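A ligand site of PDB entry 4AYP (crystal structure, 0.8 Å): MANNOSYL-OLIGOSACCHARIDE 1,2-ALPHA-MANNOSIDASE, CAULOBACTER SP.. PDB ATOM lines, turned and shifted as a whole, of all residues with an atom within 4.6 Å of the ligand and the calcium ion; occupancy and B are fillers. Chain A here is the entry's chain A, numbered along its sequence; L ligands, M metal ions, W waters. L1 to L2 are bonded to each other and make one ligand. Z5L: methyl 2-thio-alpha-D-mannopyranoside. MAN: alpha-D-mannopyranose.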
ATOM      1  N   GLN A  95      -3.576 -30.336 -29.563  1.00  0.00           N
ATOM      2  CA  GLN A  95      -2.811 -29.843 -28.440  1.00  0.00           C
ATOM      3  C   GLN A  95      -3.625 -28.703 -27.793  1.00  0.00           C
ATOM      4  O   GLN A  95      -3.932 -27.686 -28.446  1.00  0.00           O
ATOM      5  CB  GLN A  95      -1.457 -29.318 -28.900  1.00  0.00           C
ATOM      6  CG  GLN A  95      -0.503 -29.107 -27.753  1.00  0.00           C
ATOM      7  CD  GLN A  95       0.798 -28.464 -28.196  1.00  0.00           C
ATOM      8  OE1 GLN A  95       1.157 -28.461 -29.373  1.00  0.00           O
ATOM      9  NE2 GLN A  95       1.523 -27.897 -27.245  1.00  0.00           N
ATOM     10  N   PHE A  97      -3.183 -26.324 -25.493  1.00  0.00           N
ATOM     11  CA  PHE A  97      -2.624 -24.985 -25.415  1.00  0.00           C
ATOM     12  C   PHE A  97      -2.737 -24.254 -26.752  1.00  0.00           C
ATOM     13  O   PHE A  97      -3.215 -23.113 -26.827  1.00  0.00           O
ATOM     14  CB  PHE A  97      -1.156 -25.114 -24.985  1.00  0.00           C
ATOM     15  CG  PHE A  97      -0.321 -23.878 -25.185  1.00  0.00           C
ATOM     16  CD1 PHE A  97      -0.344 -22.829 -24.289  1.00  0.00           C
ATOM     17  CD2 PHE A  97       0.544 -23.805 -26.273  1.00  0.00           C
ATOM     18  CE1 PHE A  97       0.466 -21.702 -24.490  1.00  0.00           C
ATOM     19  CE2 PHE A  97       1.343 -22.681 -26.481  1.00  0.00           C
ATOM     20  CZ  PHE A  97       1.300 -21.633 -25.582  1.00  0.00           C
ATOM     21  N   GLU A  98      -2.262 -24.905 -27.822  1.00  0.00           N
ATOM     22  CA  GLU A  98      -2.246 -24.259 -29.135  1.00  0.00           C
ATOM     23  C   GLU A  98      -3.688 -24.009 -29.623  1.00  0.00           C
ATOM     24  O   GLU A  98      -3.981 -22.981 -30.250  1.00  0.00           O
ATOM     25  CB  GLU A  98      -1.512 -25.125 -30.161  1.00  0.00           C
ATOM     26  CG  GLU A  98      -0.027 -25.302 -29.899  1.00  0.00           C
ATOM     27  CD  GLU A  98       0.825 -24.049 -30.118  1.00  0.00           C
ATOM     28  OE1 GLU A  98       0.271 -23.001 -30.525  1.00  0.00           O
ATOM     29  OE2 GLU A  98       2.044 -24.143 -29.851  1.00  0.00           O
ATOM     30  N   ILE A 101      -5.043 -20.865 -27.673  1.00  0.00           N
ATOM     31  CA  ILE A 101      -4.527 -19.526 -27.944  1.00  0.00           C
ATOM     32  C   ILE A 101      -4.746 -19.138 -29.409  1.00  0.00           C
ATOM     33  O   ILE A 101      -4.906 -17.952 -29.715  1.00  0.00           O
ATOM     34  CB  ILE A 101      -3.054 -19.326 -27.517  1.00  0.00           C
ATOM     35  CG1 ILE A 101      -2.069 -20.150 -28.346  1.00  0.00           C
ATOM     36  CG2 ILE A 101      -2.909 -19.561 -26.023  1.00  0.00           C
ATOM     37  CD1 ILE A 101      -0.611 -19.793 -28.104  1.00  0.00           C
ATOM     38  N   ARG A 102      -4.779 -20.114 -30.324  1.00  0.00           N
ATOM     39  CA  ARG A 102      -4.906 -19.820 -31.746  1.00  0.00           C
ATOM     40  C   ARG A 102      -6.362 -19.804 -32.200  1.00  0.00           C
ATOM     41  O   ARG A 102      -6.808 -18.844 -32.857  1.00  0.00           O
ATOM     42  CB  ARG A 102      -4.128 -20.819 -32.590  1.00  0.00           C
ATOM     43  CG  ARG A 102      -2.633 -20.761 -32.329  1.00  0.00           C
ATOM     44  CD  ARG A 102      -1.909 -21.818 -33.081  1.00  0.00           C
ATOM     45  NE  ARG A 102      -0.468 -21.855 -32.864  1.00  0.00           N
ATOM     46  CZ  ARG A 102       0.434 -21.628 -33.798  1.00  0.00           C
ATOM     47  NH1 ARG A 102       0.102 -21.081 -34.963  1.00  0.00           N
ATOM     48  NH2 ARG A 102       1.698 -21.929 -33.557  1.00  0.00           N
ATOM     49  N   ASN A 159       3.510 -28.263 -18.554  1.00  0.00           N
ATOM     50  CA  ASN A 159       4.364 -27.147 -18.198  1.00  0.00           C
ATOM     51  C   ASN A 159       3.485 -25.946 -17.897  1.00  0.00           C
ATOM     52  O   ASN A 159       2.293 -25.927 -18.206  1.00  0.00           O
ATOM     53  CB  ASN A 159       5.411 -26.879 -19.296  1.00  0.00           C
ATOM     54  CG  ASN A 159       4.752 -26.617 -20.634  1.00  0.00           C
ATOM     55  OD1 ASN A 159       4.136 -25.559 -20.843  1.00  0.00           O
ATOM     56  ND2 ASN A 159       4.878 -27.570 -21.558  1.00  0.00           N
ATOM     57  N   ALA A 161       3.250 -22.930 -19.154  1.00  0.00           N
ATOM     58  CA  ALA A 161       2.566 -22.285 -20.275  1.00  0.00           C
ATOM     59  C   ALA A 161       1.329 -23.100 -20.668  1.00  0.00           C
ATOM     60  O   ALA A 161       0.233 -22.540 -20.920  1.00  0.00           O
ATOM     61  CB  ALA A 161       3.493 -22.100 -21.455  1.00  0.00           C
ATOM     62  N   GLU A 162       1.468 -24.421 -20.740  1.00  0.00           N
ATOM     63  CA  GLU A 162       0.401 -25.274 -21.228  1.00  0.00           C
ATOM     64  C   GLU A 162      -0.661 -25.592 -20.174  1.00  0.00           C
ATOM     65  O   GLU A 162      -1.692 -26.175 -20.541  1.00  0.00           O
ATOM     66  CB  GLU A 162       0.945 -26.541 -21.889  1.00  0.00           C
ATOM     67  CG  GLU A 162       1.787 -26.212 -23.121  1.00  0.00           C
ATOM     68  CD  GLU A 162       2.190 -27.449 -23.903  1.00  0.00           C
ATOM     69  OE1 GLU A 162       1.325 -28.307 -24.191  1.00  0.00           O
ATOM     70  OE2 GLU A 162       3.409 -27.556 -24.242  1.00  0.00           O
ATOM     71  N   VAL A 223      10.464 -20.358 -22.838  1.00  0.00           N
ATOM     72  CA  VAL A 223       9.549 -21.326 -23.423  1.00  0.00           C
ATOM     73  C   VAL A 223       9.157 -22.356 -22.370  1.00  0.00           C
ATOM     74  O   VAL A 223       9.978 -22.797 -21.556  1.00  0.00           O
ATOM     75  CB  VAL A 223      10.149 -21.997 -24.675  1.00  0.00           C
ATOM     76  CG1 VAL A 223      10.394 -20.962 -25.763  1.00  0.00           C
ATOM     77  CG2 VAL A 223      11.416 -22.749 -24.354  1.00  0.00           C
ATOM     78  N   TYR A 224       7.873 -22.716 -22.398  1.00  0.00           N
ATOM     79  CA  TYR A 224       7.228 -23.649 -21.454  1.00  0.00           C
ATOM     80  C   TYR A 224       6.817 -22.997 -20.156  1.00  0.00           C
ATOM     81  O   TYR A 224       6.231 -23.659 -19.276  1.00  0.00           O
ATOM     82  CB  TYR A 224       8.017 -24.956 -21.242  1.00  0.00           C
ATOM     83  CG  TYR A 224       8.417 -25.621 -22.544  1.00  0.00           C
ATOM     84  CD1 TYR A 224       7.467 -25.959 -23.506  1.00  0.00           C
ATOM     85  CD2 TYR A 224       9.744 -25.899 -22.825  1.00  0.00           C
ATOM     86  CE1 TYR A 224       7.826 -26.523 -24.721  1.00  0.00           C
ATOM     87  CE2 TYR A 224      10.115 -26.491 -24.032  1.00  0.00           C
ATOM     88  CZ  TYR A 224       9.156 -26.803 -24.980  1.00  0.00           C
ATOM     89  OH  TYR A 224       9.516 -27.374 -26.183  1.00  0.00           O
ATOM     90  N   ALA A 225       7.033 -21.679 -20.013  1.00  0.00           N
ATOM     91  CA  ALA A 225       6.647 -20.970 -18.804  1.00  0.00           C
ATOM     92  C   ALA A 225       6.010 -19.614 -19.130  1.00  0.00           C
ATOM     93  O   ALA A 225       4.857 -19.371 -18.785  1.00  0.00           O
ATOM     94  CB  ALA A 225       7.820 -20.853 -17.835  1.00  0.00           C
ATOM     95  N   ASP A 226       6.791 -18.763 -19.804  1.00  0.00           N
ATOM     96  CA  ASP A 226       6.436 -17.449 -20.356  1.00  0.00           C
ATOM     97  C   ASP A 226       4.984 -16.974 -20.174  1.00  0.00           C
ATOM     98  O   ASP A 226       4.726 -16.099 -19.344  1.00  0.00           O
ATOM     99  CB  ASP A 226       6.940 -17.350 -21.813  1.00  0.00           C
ATOM    100  CG  ASP A 226       6.597 -18.516 -22.757  1.00  0.00           C
ATOM    101  OD1 ASP A 226       5.645 -19.282 -22.520  1.00  0.00           O
ATOM    102  OD2 ASP A 226       7.324 -18.565 -23.792  1.00  0.00           O
ATOM    103  N   GLU A 230       2.369 -13.707 -18.218  1.00  0.00           N
ATOM    104  CA  GLU A 230       1.532 -12.722 -18.907  1.00  0.00           C
ATOM    105  C   GLU A 230       0.100 -12.823 -18.430  1.00  0.00           C
ATOM    106  O   GLU A 230      -0.553 -11.800 -18.159  1.00  0.00           O
ATOM    107  CB  GLU A 230       1.527 -12.924 -20.410  1.00  0.00           C
ATOM    108  CG  GLU A 230       2.820 -12.569 -21.122  1.00  0.00           C
ATOM    109  CD  GLU A 230       2.647 -12.813 -22.609  1.00  0.00           C
ATOM    110  OE1 GLU A 230       2.721 -14.002 -23.010  1.00  0.00           O
ATOM    111  OE2 GLU A 230       2.359 -11.838 -23.357  1.00  0.00           O
ATOM    112  N   LEU A 287      11.990 -16.025 -28.002  1.00  0.00           N
ATOM    113  CA  LEU A 287      10.623 -15.850 -27.549  1.00  0.00           C
ATOM    114  C   LEU A 287      10.552 -15.146 -26.199  1.00  0.00           C
ATOM    115  O   LEU A 287       9.506 -14.584 -25.856  1.00  0.00           O
ATOM    116  CB  LEU A 287       9.870 -17.187 -27.506  1.00  0.00           C
ATOM    117  CG  LEU A 287       9.576 -17.862 -28.851  1.00  0.00           C
ATOM    118  CD1 LEU A 287      10.786 -18.529 -29.477  1.00  0.00           C
ATOM    119  CD2 LEU A 287       8.456 -18.871 -28.652  1.00  0.00           C
ATOM    120  N   ARG A 340       9.625 -15.129 -36.021  1.00  0.00           N
ATOM    121  CA  ARG A 340       9.066 -14.942 -34.705  1.00  0.00           C
ATOM    122  C   ARG A 340       8.649 -13.487 -34.420  1.00  0.00           C
ATOM    123  O   ARG A 340       9.322 -12.535 -34.838  1.00  0.00           O
ATOM    124  CB  ARG A 340      10.076 -15.372 -33.641  1.00  0.00           C
ATOM    125  CG  ARG A 340      10.396 -16.864 -33.642  1.00  0.00           C
ATOM    126  CD  ARG A 340       9.279 -17.701 -33.046  1.00  0.00           C
ATOM    127  NE  ARG A 340       9.610 -19.112 -33.153  1.00  0.00           N
ATOM    128  CZ  ARG A 340       8.799 -20.106 -32.786  1.00  0.00           C
ATOM    129  NH1 ARG A 340       7.616 -19.880 -32.238  1.00  0.00           N
ATOM    130  NH2 ARG A 340       9.197 -21.371 -33.010  1.00  0.00           N
ATOM    131  N   PRO A 341       7.576 -13.314 -33.630  1.00  0.00           N
ATOM    132  CA  PRO A 341       6.973 -11.996 -33.410  1.00  0.00           C
ATOM    133  C   PRO A 341       7.304 -11.291 -32.081  1.00  0.00           C
ATOM    134  O   PRO A 341       6.773 -10.198 -31.852  1.00  0.00           O
ATOM    135  CB  PRO A 341       5.481 -12.343 -33.404  1.00  0.00           C
ATOM    136  CG  PRO A 341       5.438 -13.654 -32.671  1.00  0.00           C
ATOM    137  CD  PRO A 341       6.618 -14.407 -33.262  1.00  0.00           C
ATOM    138  N   GLU A 342       8.112 -11.890 -31.197  1.00  0.00           N
ATOM    139  CA  GLU A 342       8.144 -11.383 -29.830  1.00  0.00           C
ATOM    140  C   GLU A 342       8.845 -10.022 -29.672  1.00  0.00           C
ATOM    141  O   GLU A 342       8.555  -9.314 -28.701  1.00  0.00           O
ATOM    142  CB  GLU A 342       8.713 -12.406 -28.845  1.00  0.00           C
ATOM    143  CG  GLU A 342       7.789 -13.611 -28.622  1.00  0.00           C
ATOM    144  CD  GLU A 342       7.825 -14.695 -29.711  1.00  0.00           C
ATOM    145  OE1 GLU A 342       8.661 -14.627 -30.654  1.00  0.00           O
ATOM    146  OE2 GLU A 342       7.045 -15.658 -29.597  1.00  0.00           O
ATOM    147  N   ASP A 345       6.202  -7.469 -30.392  1.00  0.00           N
ATOM    148  CA  ASP A 345       5.290  -7.642 -29.240  1.00  0.00           C
ATOM    149  C   ASP A 345       5.746  -6.723 -28.092  1.00  0.00           C
ATOM    150  O   ASP A 345       4.994  -5.888 -27.599  1.00  0.00           O
ATOM    151  CB  ASP A 345       5.345  -9.142 -28.858  1.00  0.00           C
ATOM    152  CG  ASP A 345       4.580  -9.553 -27.607  1.00  0.00           C
ATOM    153  OD1 ASP A 345       4.252  -8.684 -26.775  1.00  0.00           O
ATOM    154  OD2 ASP A 345       4.427 -10.779 -27.448  1.00  0.00           O
ATOM    155  N   TYR A 400       0.881 -17.996 -36.456  1.00  0.00           N
ATOM    156  CA  TYR A 400       0.978 -16.822 -35.601  1.00  0.00           C
ATOM    157  C   TYR A 400       1.382 -15.560 -36.365  1.00  0.00           C
ATOM    158  O   TYR A 400       1.071 -14.464 -35.887  1.00  0.00           O
ATOM    159  CB  TYR A 400       1.862 -17.046 -34.371  1.00  0.00           C
ATOM    160  CG  TYR A 400       3.236 -17.666 -34.640  1.00  0.00           C
ATOM    161  CD1 TYR A 400       4.277 -16.944 -35.238  1.00  0.00           C
ATOM    162  CD2 TYR A 400       3.495 -18.985 -34.255  1.00  0.00           C
ATOM    163  CE1 TYR A 400       5.528 -17.521 -35.441  1.00  0.00           C
ATOM    164  CE2 TYR A 400       4.726 -19.563 -34.456  1.00  0.00           C
ATOM    165  CZ  TYR A 400       5.735 -18.849 -35.068  1.00  0.00           C
ATOM    166  OH  TYR A 400       6.946 -19.476 -35.280  1.00  0.00           O
ATOM    167  N   GLU A 404      -0.001 -11.949 -35.194  1.00  0.00           N
ATOM    168  CA  GLU A 404       0.951 -11.212 -34.368  1.00  0.00           C
ATOM    169  C   GLU A 404       1.702 -10.086 -35.097  1.00  0.00           C
ATOM    170  O   GLU A 404       1.307  -8.924 -34.954  1.00  0.00           O
ATOM    171  CB  GLU A 404       1.910 -12.159 -33.667  1.00  0.00           C
ATOM    172  CG  GLU A 404       1.197 -13.102 -32.700  1.00  0.00           C
ATOM    173  CD  GLU A 404       2.086 -13.613 -31.591  1.00  0.00           C
ATOM    174  OE1 GLU A 404       2.755 -12.760 -30.931  1.00  0.00           O
ATOM    175  OE2 GLU A 404       2.131 -14.838 -31.394  1.00  0.00           O
ATOM    176  N   THR A 428      -1.725 -13.656 -25.738  1.00  0.00           N
ATOM    177  CA  THR A 428      -0.331 -13.994 -26.059  1.00  0.00           C
ATOM    178  C   THR A 428      -0.124 -14.337 -27.539  1.00  0.00           C
ATOM    179  O   THR A 428       1.016 -14.418 -27.995  1.00  0.00           O
ATOM    180  CB  THR A 428       0.191 -15.135 -25.153  1.00  0.00           C
ATOM    181  OG1 THR A 428       1.615 -15.131 -25.174  1.00  0.00           O
ATOM    182  CG2 THR A 428      -0.307 -16.507 -25.581  1.00  0.00           C
ATOM    183  N   GLU A 429      -1.236 -14.541 -28.259  1.00  0.00           N
ATOM    184  CA  GLU A 429      -1.284 -14.750 -29.711  1.00  0.00           C
ATOM    185  C   GLU A 429      -1.716 -13.465 -30.446  1.00  0.00           C
ATOM    186  O   GLU A 429      -2.055 -13.490 -31.626  1.00  0.00           O
ATOM    187  CB  GLU A 429      -2.269 -15.899 -30.006  1.00  0.00           C
ATOM    188  CG  GLU A 429      -2.232 -16.477 -31.410  1.00  0.00           C
ATOM    189  CD  GLU A 429      -1.052 -17.382 -31.709  1.00  0.00           C
ATOM    190  OE1 GLU A 429      -0.289 -17.739 -30.789  1.00  0.00           O
ATOM    191  OE2 GLU A 429      -0.889 -17.810 -32.905  1.00  0.00           O
HETATM  192  S2  Z5L L   1       3.985 -20.467 -28.035  1.00  0.00           S
HETATM  193  C2  Z5L L   1       5.653 -21.027 -27.614  1.00  0.00           C
HETATM  194  C1  Z5L L   1       5.741 -22.521 -27.947  1.00  0.00           C
HETATM  195  O1  Z5L L   1       7.103 -22.911 -27.891  1.00  0.00           O
HETATM  196  C1M Z5L L   1       7.277 -24.311 -28.164  1.00  0.00           C
HETATM  197  O5  Z5L L   1       4.939 -23.296 -27.051  1.00  0.00           O
HETATM  198  C3  Z5L L   1       6.020 -20.841 -26.132  1.00  0.00           C
HETATM  199  O3  Z5L L   1       5.832 -19.471 -25.761  1.00  0.00           O
HETATM  200  C4  Z5L L   1       5.218 -21.744 -25.210  1.00  0.00           C
HETATM  201  O4  Z5L L   1       5.720 -21.671 -23.876  1.00  0.00           O
HETATM  202  C5  Z5L L   1       5.333 -23.189 -25.683  1.00  0.00           C
HETATM  203  C6  Z5L L   1       4.439 -24.135 -24.916  1.00  0.00           C
HETATM  204  O6  Z5L L   1       4.666 -25.461 -25.416  1.00  0.00           O
HETATM  205  C1  MAN L   2       4.205 -18.667 -28.187  1.00  0.00           C
HETATM  206  C2  MAN L   2       2.789 -18.028 -28.124  1.00  0.00           C
HETATM  207  C3  MAN L   2       2.484 -17.181 -29.349  1.00  0.00           C
HETATM  208  C4  MAN L   2       2.864 -17.941 -30.613  1.00  0.00           C
HETATM  209  C5  MAN L   2       4.357 -18.297 -30.619  1.00  0.00           C
HETATM  210  C6  MAN L   2       5.114 -17.277 -31.471  1.00  0.00           C
HETATM  211  O2  MAN L   2       2.649 -17.182 -26.987  1.00  0.00           O
HETATM  212  O3  MAN L   2       3.193 -15.948 -29.252  1.00  0.00           O
HETATM  213  O4  MAN L   2       2.102 -19.142 -30.725  1.00  0.00           O
HETATM  214  O5  MAN L   2       4.976 -18.235 -29.319  1.00  0.00           O
HETATM  215  O6  MAN L   2       6.524 -17.459 -31.443  1.00  0.00           O
HETATM  216 CA    CA M   1       3.275 -14.825 -27.033  1.00  0.00          CA
HETATM  217  O   HOH W   1       3.167 -18.843 -24.988  1.00  0.00           O
HETATM  218  O   HOH W   2       3.094 -21.860 -31.065  1.00  0.00           O
HETATM  219  O   HOH W   3       3.458 -25.844 -28.033  1.00  0.00           O
HETATM  220  O   HOH W   4       2.961 -12.620 -26.039  1.00  0.00           O
HETATM  221  O   HOH W   5       8.048 -23.455 -31.383  1.00  0.00           O
HETATM  222  O   HOH W   6       4.470 -15.079 -24.890  1.00  0.00           O
HETATM  223  O   HOH W   7       5.457 -15.732 -27.403  1.00  0.00           O
HETATM  224  O   HOH W   8       9.721 -22.392 -29.443  1.00  0.00           O
HETATM  225  O   HOH W   9       4.170 -13.229 -28.673  1.00  0.00           O
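Merely in contact with the ligand: Ala 161 (3.3 Å), Pro 341 (3.6 Å), Leu 287 (3.6 Å), Tyr 400 (3.6 Å), Phe 97 (3.7 Å), Val 223 (3.8 Å), Ile 101 (3.8 Å) and Arg 102 (3.99 Å). Hydrophobic or aromatic side chains within 4 Å of the ligand: Phe 97, Ile 101, Ala 161, Tyr 224, Leu 287, Pro 341 and Tyr 400. 16 residues have an atom within 4 Å of the ligand: Phe 97, Ile 101, Arg 102, Ala 161, Glu 162, Val 223, Tyr 224, Asp 226, Leu 287, Arg 340, Pro 341, Glu 342, Tyr 400, Glu 404, Thr 428 and Glu 429. The nearest printed residue that does not touch the ligand is Ala 225 (4.1 Å).
The side-chain hydroxyl of Tyr 400 sits at hydrogen-bond distance from the guanidinium group of Arg 340. The backbone carbonyl oxygen (O) of Tyr 224 lies close to the side-chain amide oxygen (OD1) of Asn 159, 3.2 Å away. The backbone NH (N) of Ala 161 is in hydrogen-bond range of the side-chain amide oxygen (OD1) of Asn 159, 3.2 Å away. The side-chain amide oxygen (OD1) of Asn 159 sits at hydrogen-bond distance from the backbone NH (N) of Glu 162, 2.9 Å away. The side-chain hydroxyl (OG1) of Thr 428 lies close to the side-chain carboxylate (OE1) of Glu 230 (2.7 Å). The guanidinium group (NE) of Arg 102 is in salt-bridge range of the side-chain carboxylate (OE1) of Glu 98, 2.7 Å away. The side-chain carboxylate (OE1) of Glu 162 lies within hydrogen-bond range of the side-chain amide nitrogen (NE2) of Gln 95, 3.1 Å away. OE2 of Glu 429 is in salt-bridge range of NH1 of Arg 102, 3.99 Å away.
Water W4 bridges OD2 of Asp 345 and OE1 of Glu 230. Water W9 lies within hydrogen-bond range of OE1 of Glu 404 (2.7 Å) and OD2 of Asp 345 (2.8 Å). Water W7 bridges OE2 of Glu 342 and O5 of MAN L2. Water W3 lies within hydrogen-bond range of the side-chain carboxylate of Glu 98 (2.9 Å), an oxygen (O6) of Z5L L1 (2.9 Å) and the side-chain amide nitrogen of Gln 95 (2.9 Å). Water W2 lies within hydrogen-bond range of OE2 of Glu 98 (2.8 Å), NH2 of Arg 102 (2.9 Å) and O4 of MAN L2 (2.9 Å).
The side-chain carboxylate (OE2) of Glu 404 lies close to an oxygen (O3) of MAN L2, 2.6 Å away. An oxygen (O6) of MAN L2 lies within hydrogen-bond range of the guanidinium group of Arg 340, 2.8 Å away. O6 of Z5L L1 lies within hydrogen-bond range of OE2 of Glu 162 (2.7 Å). The side-chain carboxylate (OD2) of Asp 226 lies within hydrogen-bond range of an oxygen (O3) of Z5L L1. An oxygen (O4) of Z5L L1 is in hydrogen-bond range of the backbone NH (N) of Tyr 224. The side-chain carboxylate (OE2) of Glu 342 is in hydrogen-bond range of an oxygen (O6) of MAN L2. The side-chain carboxylate of Glu 429 sits at hydrogen-bond distance from an oxygen (O4) of MAN L2 (2.8 Å).
The calcium ion is bound by water W7, O2 of MAN L2, water W4, water W9, water W6, O3 of MAN L2, O of Thr 428 and OG1 of Thr 428.
Of the 22 residues printed, 1 comes within 4 Å of the calcium ion.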
